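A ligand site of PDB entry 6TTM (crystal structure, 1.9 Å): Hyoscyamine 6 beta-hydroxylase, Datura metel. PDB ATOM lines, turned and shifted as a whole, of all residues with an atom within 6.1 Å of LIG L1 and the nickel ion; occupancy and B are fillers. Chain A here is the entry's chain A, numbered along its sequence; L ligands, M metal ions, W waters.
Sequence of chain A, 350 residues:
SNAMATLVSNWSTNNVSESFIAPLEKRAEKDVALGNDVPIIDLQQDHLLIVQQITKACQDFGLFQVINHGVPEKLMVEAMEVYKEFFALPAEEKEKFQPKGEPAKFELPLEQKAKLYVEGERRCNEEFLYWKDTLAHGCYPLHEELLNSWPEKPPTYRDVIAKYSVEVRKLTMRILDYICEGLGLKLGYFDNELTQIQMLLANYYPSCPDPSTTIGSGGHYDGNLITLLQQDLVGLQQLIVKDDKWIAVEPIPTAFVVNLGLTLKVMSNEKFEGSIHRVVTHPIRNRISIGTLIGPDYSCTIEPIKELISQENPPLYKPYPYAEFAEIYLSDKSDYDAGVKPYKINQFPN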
ATOM      1  N   GLU A 119      -3.890  24.879  -4.539  1.00  0.00           N
ATOM      2  CA  GLU A 119      -3.906  23.449  -4.880  1.00  0.00           C
ATOM      3  C   GLU A 119      -5.288  22.879  -4.536  1.00  0.00           C
ATOM      4  O   GLU A 119      -5.582  22.636  -3.372  1.00  0.00           O
ATOM      5  CB  GLU A 119      -2.789  22.729  -4.085  1.00  0.00           C
ATOM      6  CG  GLU A 119      -2.461  21.346  -4.684  1.00  0.00           C
ATOM      7  CD  GLU A 119      -1.270  20.709  -4.017  1.00  0.00           C
ATOM      8  OE1 GLU A 119      -0.783  21.256  -3.014  1.00  0.00           O
ATOM      9  OE2 GLU A 119      -0.822  19.652  -4.510  1.00  0.00           O
ATOM     10  N   LYS A 132      -6.243  26.290   0.697  1.00  0.00           N
ATOM     11  CA  LYS A 132      -4.829  26.341   1.122  1.00  0.00           C
ATOM     12  C   LYS A 132      -4.146  27.371   0.242  1.00  0.00           C
ATOM     13  O   LYS A 132      -4.252  27.291  -0.984  1.00  0.00           O
ATOM     14  CB  LYS A 132      -4.128  24.959   0.955  1.00  0.00           C
ATOM     15  CG  LYS A 132      -2.550  25.038   1.178  1.00  0.00           C
ATOM     16  CD  LYS A 132      -1.894  23.620   1.124  1.00  0.00           C
ATOM     17  CE  LYS A 132      -2.036  23.070  -0.299  1.00  0.00           C
ATOM     18  NZ  LYS A 132      -0.865  22.328  -0.710  1.00  0.00           N
ATOM     19  N   LEU A 201       7.838  25.264   1.113  1.00  0.00           N
ATOM     20  CA  LEU A 201       6.402  25.424   0.880  1.00  0.00           C
ATOM     21  C   LEU A 201       5.804  25.831   2.217  1.00  0.00           C
ATOM     22  O   LEU A 201       5.674  24.975   3.098  1.00  0.00           O
ATOM     23  CB  LEU A 201       5.732  24.127   0.379  1.00  0.00           C
ATOM     24  CG  LEU A 201       5.735  23.936  -1.125  1.00  0.00           C
ATOM     25  CD1 LEU A 201       7.174  23.780  -1.592  1.00  0.00           C
ATOM     26  CD2 LEU A 201       4.867  22.647  -1.551  1.00  0.00           C
ATOM     27  N   ASN A 203       2.544  26.913   4.146  1.00  0.00           N
ATOM     28  CA  ASN A 203       1.113  26.683   3.870  1.00  0.00           C
ATOM     29  C   ASN A 203       0.240  27.371   4.889  1.00  0.00           C
ATOM     30  O   ASN A 203       0.548  27.371   6.090  1.00  0.00           O
ATOM     31  CB  ASN A 203       0.783  25.181   3.941  1.00  0.00           C
ATOM     32  CG  ASN A 203       1.728  24.385   3.155  1.00  0.00           C
ATOM     33  OD1 ASN A 203       1.772  24.523   1.947  1.00  0.00           O
ATOM     34  ND2 ASN A 203       2.537  23.546   3.838  1.00  0.00           N
ATOM     35  N   TYR A 205      -3.813  27.428   6.020  1.00  0.00           N
ATOM     36  CA  TYR A 205      -5.098  26.737   5.910  1.00  0.00           C
ATOM     37  C   TYR A 205      -6.129  27.521   6.685  1.00  0.00           C
ATOM     38  O   TYR A 205      -6.109  27.504   7.930  1.00  0.00           O
ATOM     39  CB  TYR A 205      -5.022  25.328   6.481  1.00  0.00           C
ATOM     40  CG  TYR A 205      -3.966  24.488   5.887  1.00  0.00           C
ATOM     41  CD1 TYR A 205      -4.261  23.732   4.745  1.00  0.00           C
ATOM     42  CD2 TYR A 205      -2.662  24.388   6.457  1.00  0.00           C
ATOM     43  CE1 TYR A 205      -3.270  22.899   4.205  1.00  0.00           C
ATOM     44  CE2 TYR A 205      -1.681  23.567   5.885  1.00  0.00           C
ATOM     45  CZ  TYR A 205      -1.997  22.843   4.748  1.00  0.00           C
ATOM     46  OH  TYR A 205      -1.033  22.008   4.157  1.00  0.00           O
ATOM     47  N   HIS A 220      -1.694  12.483  -0.158  1.00  0.00           N
ATOM     48  CA  HIS A 220      -0.661  12.380  -1.178  1.00  0.00           C
ATOM     49  C   HIS A 220       0.596  11.747  -0.562  1.00  0.00           C
ATOM     50  O   HIS A 220       0.822  11.820   0.658  1.00  0.00           O
ATOM     51  CB  HIS A 220      -0.290  13.759  -1.751  1.00  0.00           C
ATOM     52  CG  HIS A 220       0.195  14.723  -0.695  1.00  0.00           C
ATOM     53  ND1 HIS A 220      -0.682  15.397   0.154  1.00  0.00           N
ATOM     54  CD2 HIS A 220       1.449  15.102  -0.325  1.00  0.00           C
ATOM     55  CE1 HIS A 220       0.030  16.105   1.019  1.00  0.00           C
ATOM     56  NE2 HIS A 220       1.318  15.981   0.729  1.00  0.00           N
ATOM     57  N   TYR A 221       1.440  11.194  -1.417  1.00  0.00           N
ATOM     58  CA  TYR A 221       2.872  11.143  -1.129  1.00  0.00           C
ATOM     59  C   TYR A 221       3.430  12.483  -1.538  1.00  0.00           C
ATOM     60  O   TYR A 221       2.979  13.076  -2.525  1.00  0.00           O
ATOM     61  CB  TYR A 221       3.600  10.151  -2.010  1.00  0.00           C
ATOM     62  CG  TYR A 221       3.314   8.709  -1.816  1.00  0.00           C
ATOM     63  CD1 TYR A 221       3.905   8.020  -0.763  1.00  0.00           C
ATOM     64  CD2 TYR A 221       2.495   8.012  -2.690  1.00  0.00           C
ATOM     65  CE1 TYR A 221       3.682   6.649  -0.602  1.00  0.00           C
ATOM     66  CE2 TYR A 221       2.256   6.646  -2.540  1.00  0.00           C
ATOM     67  CZ  TYR A 221       2.821   5.986  -1.475  1.00  0.00           C
ATOM     68  OH  TYR A 221       2.569   4.616  -1.310  1.00  0.00           O
ATOM     69  N   ASP A 222       4.498  12.916  -0.866  1.00  0.00           N
ATOM     70  CA  ASP A 222       5.344  13.938  -1.485  1.00  0.00           C
ATOM     71  C   ASP A 222       6.167  13.267  -2.569  1.00  0.00           C
ATOM     72  O   ASP A 222       6.744  12.197  -2.332  1.00  0.00           O
ATOM     73  CB  ASP A 222       6.298  14.530  -0.458  1.00  0.00           C
ATOM     74  CG  ASP A 222       5.592  15.392   0.608  1.00  0.00           C
ATOM     75  OD1 ASP A 222       4.394  15.707   0.490  1.00  0.00           O
ATOM     76  OD2 ASP A 222       6.277  15.803   1.565  1.00  0.00           O
ATOM     77  N   THR A 227      11.104  15.076   3.047  1.00  0.00           N
ATOM     78  CA  THR A 227      10.493  16.369   3.414  1.00  0.00           C
ATOM     79  C   THR A 227      10.583  16.574   4.921  1.00  0.00           C
ATOM     80  O   THR A 227      10.351  15.622   5.672  1.00  0.00           O
ATOM     81  CB  THR A 227       9.015  16.417   2.963  1.00  0.00           C
ATOM     82  OG1 THR A 227       8.965  16.344   1.530  1.00  0.00           O
ATOM     83  CG2 THR A 227       8.290  17.738   3.457  1.00  0.00           C
ATOM     84  N   LEU A 229       8.896  18.957   7.944  1.00  0.00           N
ATOM     85  CA  LEU A 229       7.735  19.815   8.087  1.00  0.00           C
ATOM     86  C   LEU A 229       7.692  20.342   9.519  1.00  0.00           C
ATOM     87  O   LEU A 229       7.870  19.571  10.462  1.00  0.00           O
ATOM     88  CB  LEU A 229       6.476  18.977   7.726  1.00  0.00           C
ATOM     89  CG  LEU A 229       5.052  19.506   7.707  1.00  0.00           C
ATOM     90  CD1 LEU A 229       4.494  19.803   9.046  1.00  0.00           C
ATOM     91  CD2 LEU A 229       4.879  20.649   6.702  1.00  0.00           C
ATOM     92  N   GLN A 231       5.297  22.261  12.308  1.00  0.00           N
ATOM     93  CA  GLN A 231       3.898  22.628  12.561  1.00  0.00           C
ATOM     94  C   GLN A 231       3.760  22.925  14.032  1.00  0.00           C
ATOM     95  O   GLN A 231       4.568  22.472  14.855  1.00  0.00           O
ATOM     96  CB  GLN A 231       2.894  21.459  12.214  1.00  0.00           C
ATOM     97  CG  GLN A 231       3.380  20.095  12.882  1.00  0.00           C
ATOM     98  CD  GLN A 231       2.298  19.007  12.859  1.00  0.00           C
ATOM     99  OE1 GLN A 231       1.255  19.215  12.235  1.00  0.00           O
ATOM    100  NE2 GLN A 231       2.567  17.826  13.502  1.00  0.00           N
ATOM    101  N   GLY A 235      -3.626  18.905  12.581  1.00  0.00           N
ATOM    102  CA  GLY A 235      -4.202  18.961  11.246  1.00  0.00           C
ATOM    103  C   GLY A 235      -3.543  17.945  10.325  1.00  0.00           C
ATOM    104  O   GLY A 235      -4.179  17.496   9.372  1.00  0.00           O
ATOM    105  N   LEU A 236      -2.293  17.545  10.611  1.00  0.00           N
ATOM    106  CA  LEU A 236      -1.575  16.624   9.741  1.00  0.00           C
ATOM    107  C   LEU A 236      -1.943  15.206  10.155  1.00  0.00           C
ATOM    108  O   LEU A 236      -2.008  14.904  11.351  1.00  0.00           O
ATOM    109  CB  LEU A 236      -0.065  16.842   9.824  1.00  0.00           C
ATOM    110  CG  LEU A 236       0.844  15.847   9.097  1.00  0.00           C
ATOM    111  CD1 LEU A 236       0.772  15.941   7.614  1.00  0.00           C
ATOM    112  CD2 LEU A 236       2.331  15.996   9.588  1.00  0.00           C
ATOM    113  N   ASN A 259       9.101  13.154   6.518  1.00  0.00           N
ATOM    114  CA  ASN A 259       8.378  12.126   5.780  1.00  0.00           C
ATOM    115  C   ASN A 259       9.143  11.798   4.515  1.00  0.00           C
ATOM    116  O   ASN A 259       9.679  12.684   3.832  1.00  0.00           O
ATOM    117  CB  ASN A 259       6.931  12.501   5.451  1.00  0.00           C
ATOM    118  CG  ASN A 259       6.857  13.589   4.462  1.00  0.00           C
ATOM    119  OD1 ASN A 259       6.961  14.746   4.839  1.00  0.00           O
ATOM    120  ND2 ASN A 259       6.674  13.255   3.189  1.00  0.00           N
ATOM    121  N   HIS A 277      -0.020  11.091   3.480  1.00  0.00           N
ATOM    122  CA  HIS A 277      -0.418  11.983   4.550  1.00  0.00           C
ATOM    123  C   HIS A 277      -1.368  13.044   3.961  1.00  0.00           C
ATOM    124  O   HIS A 277      -1.460  13.221   2.728  1.00  0.00           O
ATOM    125  CB  HIS A 277       0.826  12.628   5.221  1.00  0.00           C
ATOM    126  CG  HIS A 277       1.719  13.355   4.257  1.00  0.00           C
ATOM    127  ND1 HIS A 277       2.776  12.760   3.600  1.00  0.00           N
ATOM    128  CD2 HIS A 277       1.707  14.660   3.845  1.00  0.00           C
ATOM    129  CE1 HIS A 277       3.367  13.666   2.820  1.00  0.00           C
ATOM    130  NE2 HIS A 277       2.703  14.818   2.938  1.00  0.00           N
ATOM    131  N   ARG A 278      -2.107  13.720   4.835  1.00  0.00           N
ATOM    132  CA  ARG A 278      -3.074  14.741   4.421  1.00  0.00           C
ATOM    133  C   ARG A 278      -3.215  15.783   5.528  1.00  0.00           C
ATOM    134  O   ARG A 278      -2.695  15.612   6.631  1.00  0.00           O
ATOM    135  CB  ARG A 278      -4.448  14.099   4.127  1.00  0.00           C
ATOM    136  CG  ARG A 278      -5.189  13.598   5.384  1.00  0.00           C
ATOM    137  CD  ARG A 278      -6.591  13.064   5.003  1.00  0.00           C
ATOM    138  NE  ARG A 278      -7.355  12.703   6.200  1.00  0.00           N
ATOM    139  CZ  ARG A 278      -8.573  12.167   6.207  1.00  0.00           C
ATOM    140  NH1 ARG A 278      -9.211  11.861   5.064  1.00  0.00           N
ATOM    141  NH2 ARG A 278      -9.160  11.912   7.372  1.00  0.00           N
ATOM    142  N   VAL A 279      -3.931  16.878   5.245  1.00  0.00           N
ATOM    143  CA  VAL A 279      -4.175  17.907   6.259  1.00  0.00           C
ATOM    144  C   VAL A 279      -5.662  18.099   6.397  1.00  0.00           C
ATOM    145  O   VAL A 279      -6.366  18.221   5.377  1.00  0.00           O
ATOM    146  CB  VAL A 279      -3.505  19.260   5.882  1.00  0.00           C
ATOM    147  CG1 VAL A 279      -3.862  20.307   6.898  1.00  0.00           C
ATOM    148  CG2 VAL A 279      -2.012  19.094   5.851  1.00  0.00           C
ATOM    149  N   ARG A 287      -4.281  27.673  10.252  1.00  0.00           N
ATOM    150  CA  ARG A 287      -3.104  26.887  10.564  1.00  0.00           C
ATOM    151  C   ARG A 287      -2.008  27.190   9.556  1.00  0.00           C
ATOM    152  O   ARG A 287      -2.254  27.205   8.332  1.00  0.00           O
ATOM    153  CB  ARG A 287      -3.474  25.373  10.529  1.00  0.00           C
ATOM    154  CG  ARG A 287      -2.265  24.458  10.777  1.00  0.00           C
ATOM    155  CD  ARG A 287      -2.768  22.943  10.830  1.00  0.00           C
ATOM    156  NE  ARG A 287      -1.598  22.035  10.977  1.00  0.00           N
ATOM    157  CZ  ARG A 287      -0.882  21.581   9.959  1.00  0.00           C
ATOM    158  NH1 ARG A 287      -1.222  21.914   8.693  1.00  0.00           N
ATOM    159  NH2 ARG A 287       0.140  20.733  10.174  1.00  0.00           N
ATOM    160  N   SER A 289       1.929  25.912   8.290  1.00  0.00           N
ATOM    161  CA  SER A 289       2.991  24.934   8.446  1.00  0.00           C
ATOM    162  C   SER A 289       4.096  25.263   7.454  1.00  0.00           C
ATOM    163  O   SER A 289       3.848  25.944   6.478  1.00  0.00           O
ATOM    164  CB  SER A 289       2.465  23.484   8.200  1.00  0.00           C
ATOM    165  OG  SER A 289       2.078  23.383   6.820  1.00  0.00           O
ATOM    166  N   ILE A 290       5.313  24.799   7.719  1.00  0.00           N
ATOM    167  CA  ILE A 290       6.459  25.114   6.907  1.00  0.00           C
ATOM    168  C   ILE A 290       7.075  23.821   6.448  1.00  0.00           C
ATOM    169  O   ILE A 290       7.639  23.066   7.269  1.00  0.00           O
ATOM    170  CB  ILE A 290       7.522  25.920   7.698  1.00  0.00           C
ATOM    171  CG1 ILE A 290       6.867  27.104   8.415  1.00  0.00           C
ATOM    172  CG2 ILE A 290       8.621  26.355   6.677  1.00  0.00           C
ATOM    173  CD1 ILE A 290       7.906  27.844   9.396  1.00  0.00           C
ATOM    174  N   GLY A 291       7.047  23.562   5.142  1.00  0.00           N
ATOM    175  CA  GLY A 291       7.634  22.347   4.587  1.00  0.00           C
ATOM    176  C   GLY A 291       8.904  22.652   3.811  1.00  0.00           C
ATOM    177  O   GLY A 291       8.952  23.593   3.006  1.00  0.00           O
ATOM    178  N   LEU A 293      10.982  20.660   1.080  1.00  0.00           N
ATOM    179  CA  LEU A 293      10.817  19.494   0.200  1.00  0.00           C
ATOM    180  C   LEU A 293      12.093  19.381  -0.599  1.00  0.00           C
ATOM    181  O   LEU A 293      12.375  20.216  -1.450  1.00  0.00           O
ATOM    182  CB  LEU A 293       9.593  19.677  -0.710  1.00  0.00           C
ATOM    183  CG  LEU A 293       8.258  19.393  -0.011  1.00  0.00           C
ATOM    184  CD1 LEU A 293       7.863  20.595   0.936  1.00  0.00           C
ATOM    185  CD2 LEU A 293       7.197  19.190  -1.152  1.00  0.00           C
HETATM  186  C1  LIG L   1       2.661  19.223   1.912  1.00  0.00           C
HETATM  187  C2  LIG L   1       2.084  18.687   3.178  1.00  0.00           C
HETATM  188  C3  LIG L   1       1.477  18.998   5.508  1.00  0.00           C
HETATM  189  C4  LIG L   1       1.046  20.132   6.472  1.00  0.00           C
HETATM  190  O1  LIG L   1       2.690  20.498   1.757  1.00  0.00           O
HETATM  191  O2  LIG L   1       3.160  18.417   1.090  1.00  0.00           O
HETATM  192  O3  LIG L   1       1.829  17.541   3.310  1.00  0.00           O
HETATM  193  O4  LIG L   1       0.965  19.918   7.693  1.00  0.00           O
HETATM  194  N1  LIG L   1       1.946  19.604   4.277  1.00  0.00           N
HETATM  195  O5  LIG L   1       0.847  21.261   6.023  1.00  0.00           O
HETATM  196  C1  LG2 L   2       2.695  20.650  -4.046  1.00  0.00           C
HETATM  197  C2  LG2 L   2       5.395  19.723  -5.344  1.00  0.00           C
HETATM  198  C3  LG2 L   2       7.208  18.262  -6.130  1.00  0.00           C
HETATM  199  C4  LG2 L   2       6.899  18.625  -7.576  1.00  0.00           C
HETATM  200  C5  LG2 L   2       8.286  16.035  -6.924  1.00  0.00           C
HETATM  201  C6  LG2 L   2       8.000  16.414  -8.360  1.00  0.00           C
HETATM  202  C7  LG2 L   2       2.005  18.031  -3.180  1.00  0.00           C
HETATM  203  C8  LG2 L   2       2.361  20.110  -2.638  1.00  0.00           C
HETATM  204  C9  LG2 L   2       3.346  17.936  -2.332  1.00  0.00           C
HETATM  205  C10 LG2 L   2       3.602  19.364  -2.001  1.00  0.00           C
HETATM  206  C11 LG2 L   2       2.284  18.126  -4.644  1.00  0.00           C
HETATM  207  C12 LG2 L   2       3.144  19.421  -5.076  1.00  0.00           C
HETATM  208  C13 LG2 L   2       0.696  18.865  -1.560  1.00  0.00           C
HETATM  209  C14 LG2 L   2       6.801  19.263  -5.035  1.00  0.00           C
HETATM  210  C15 LG2 L   2       7.766  20.455  -5.136  1.00  0.00           C
HETATM  211  C16 LG2 L   2       7.926  16.983  -5.778  1.00  0.00           C
HETATM  212  C17 LG2 L   2       7.289  17.696  -8.719  1.00  0.00           C
HETATM  213  N1  LG2 L   2       1.420  19.151  -2.719  1.00  0.00           N
HETATM  214  O1  LG2 L   2       4.339  18.998  -4.831  1.00  0.00           O
HETATM  215  O2  LG2 L   2       5.239  20.691  -6.006  1.00  0.00           O
HETATM  216  O3  LG2 L   2       9.106  19.945  -5.035  1.00  0.00           O
HETATM  217 NI    NI M   1       3.028  16.496   1.858  1.00  0.00          NI
HETATM  218  O   HOH W   1       1.632  22.368   0.134  1.00  0.00           O
HETATM  219  O   HOH W   2       4.770  22.039   2.859  1.00  0.00           O
HETATM  220  O   HOH W   3       4.707  17.051   3.149  1.00  0.00           O
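Asn 203 touches LIG L1.
CD1 of Leu 229 touches O4 of LIG L1, 3.8 Å away.
Leu 236 touches LIG L1.
Val 279 touches LIG L1.
Hydrophobic or aromatic side chains within 4 Å of LIG L1: Tyr 205, His 220, Leu 229, Leu 236, His 277 and Val 279.
Of the 22 residues printed, 10 come within 4 Å of LIG L1.
The nearest printed residue that does not touch LIG L1 is Leu 201 (4.5 Å).
Three residues have an atom within 4 Å of the nickel ion: His 220, Asp 222 and His 277.
The nearest printed residue that does not touch the nickel ion is Asn 259 (5.1 Å).
Water W1 lies within hydrogen-bond range of NZ of Lys 132, O1 of LIG L1 and OD1 of Asn 203.
Water W2 lies within hydrogen-bond range of O1 of LIG L1, ND2 of Asn 203 and O of Leu 201.
The side-chain hydroxyl of Ser 289 is in hydrogen-bond range of an oxygen (O5) of LIG L1 (2.6 Å).
O4 of LIG L1 is in salt-bridge range of NH2 of Arg 287, at 2.7 Å.
The side-chain hydroxyl (OH) of Tyr 205 sits at hydrogen-bond distance from an oxygen (O5) of LIG L1 (2.8 Å).
OE2 of Glu 119 is in salt-bridge range of N1 of LG2 L2, 2.9 Å away.
OD2 of Asp 222 sits at hydrogen-bond distance from ND2 of Asn 259 (3.0 Å).
OD2 of Asp 222 lies within hydrogen-bond range of OG1 of Thr 227, at 2.7 Å.
The backbone carbonyl oxygen (O) of Ser 289 lies within hydrogen-bond range of the backbone NH (N) of Asn 203 (2.8 Å).
The backbone NH (N) of Tyr 205 is in hydrogen-bond range of the backbone carbonyl oxygen (O) of Arg 287, 2.8 Å away.
NH2 of Arg 287 is in hydrogen-bond range of OE1 of Gln 231, at 2.8 Å.
NE2 of His 277 is bound to the nickel ion (2.0 Å).
The nickel ion is bound by O2 of LIG L1.
OD1 of Asp 222 binds the nickel ion, at 2.1 Å.
The nickel ion is bound by NE2 of His 220 (2.1 Å).
O3 of LIG L1 binds the nickel ion.
Water W3 binds the nickel ion (2.2 Å).
The nickel ion has six donor atoms within binding distance.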
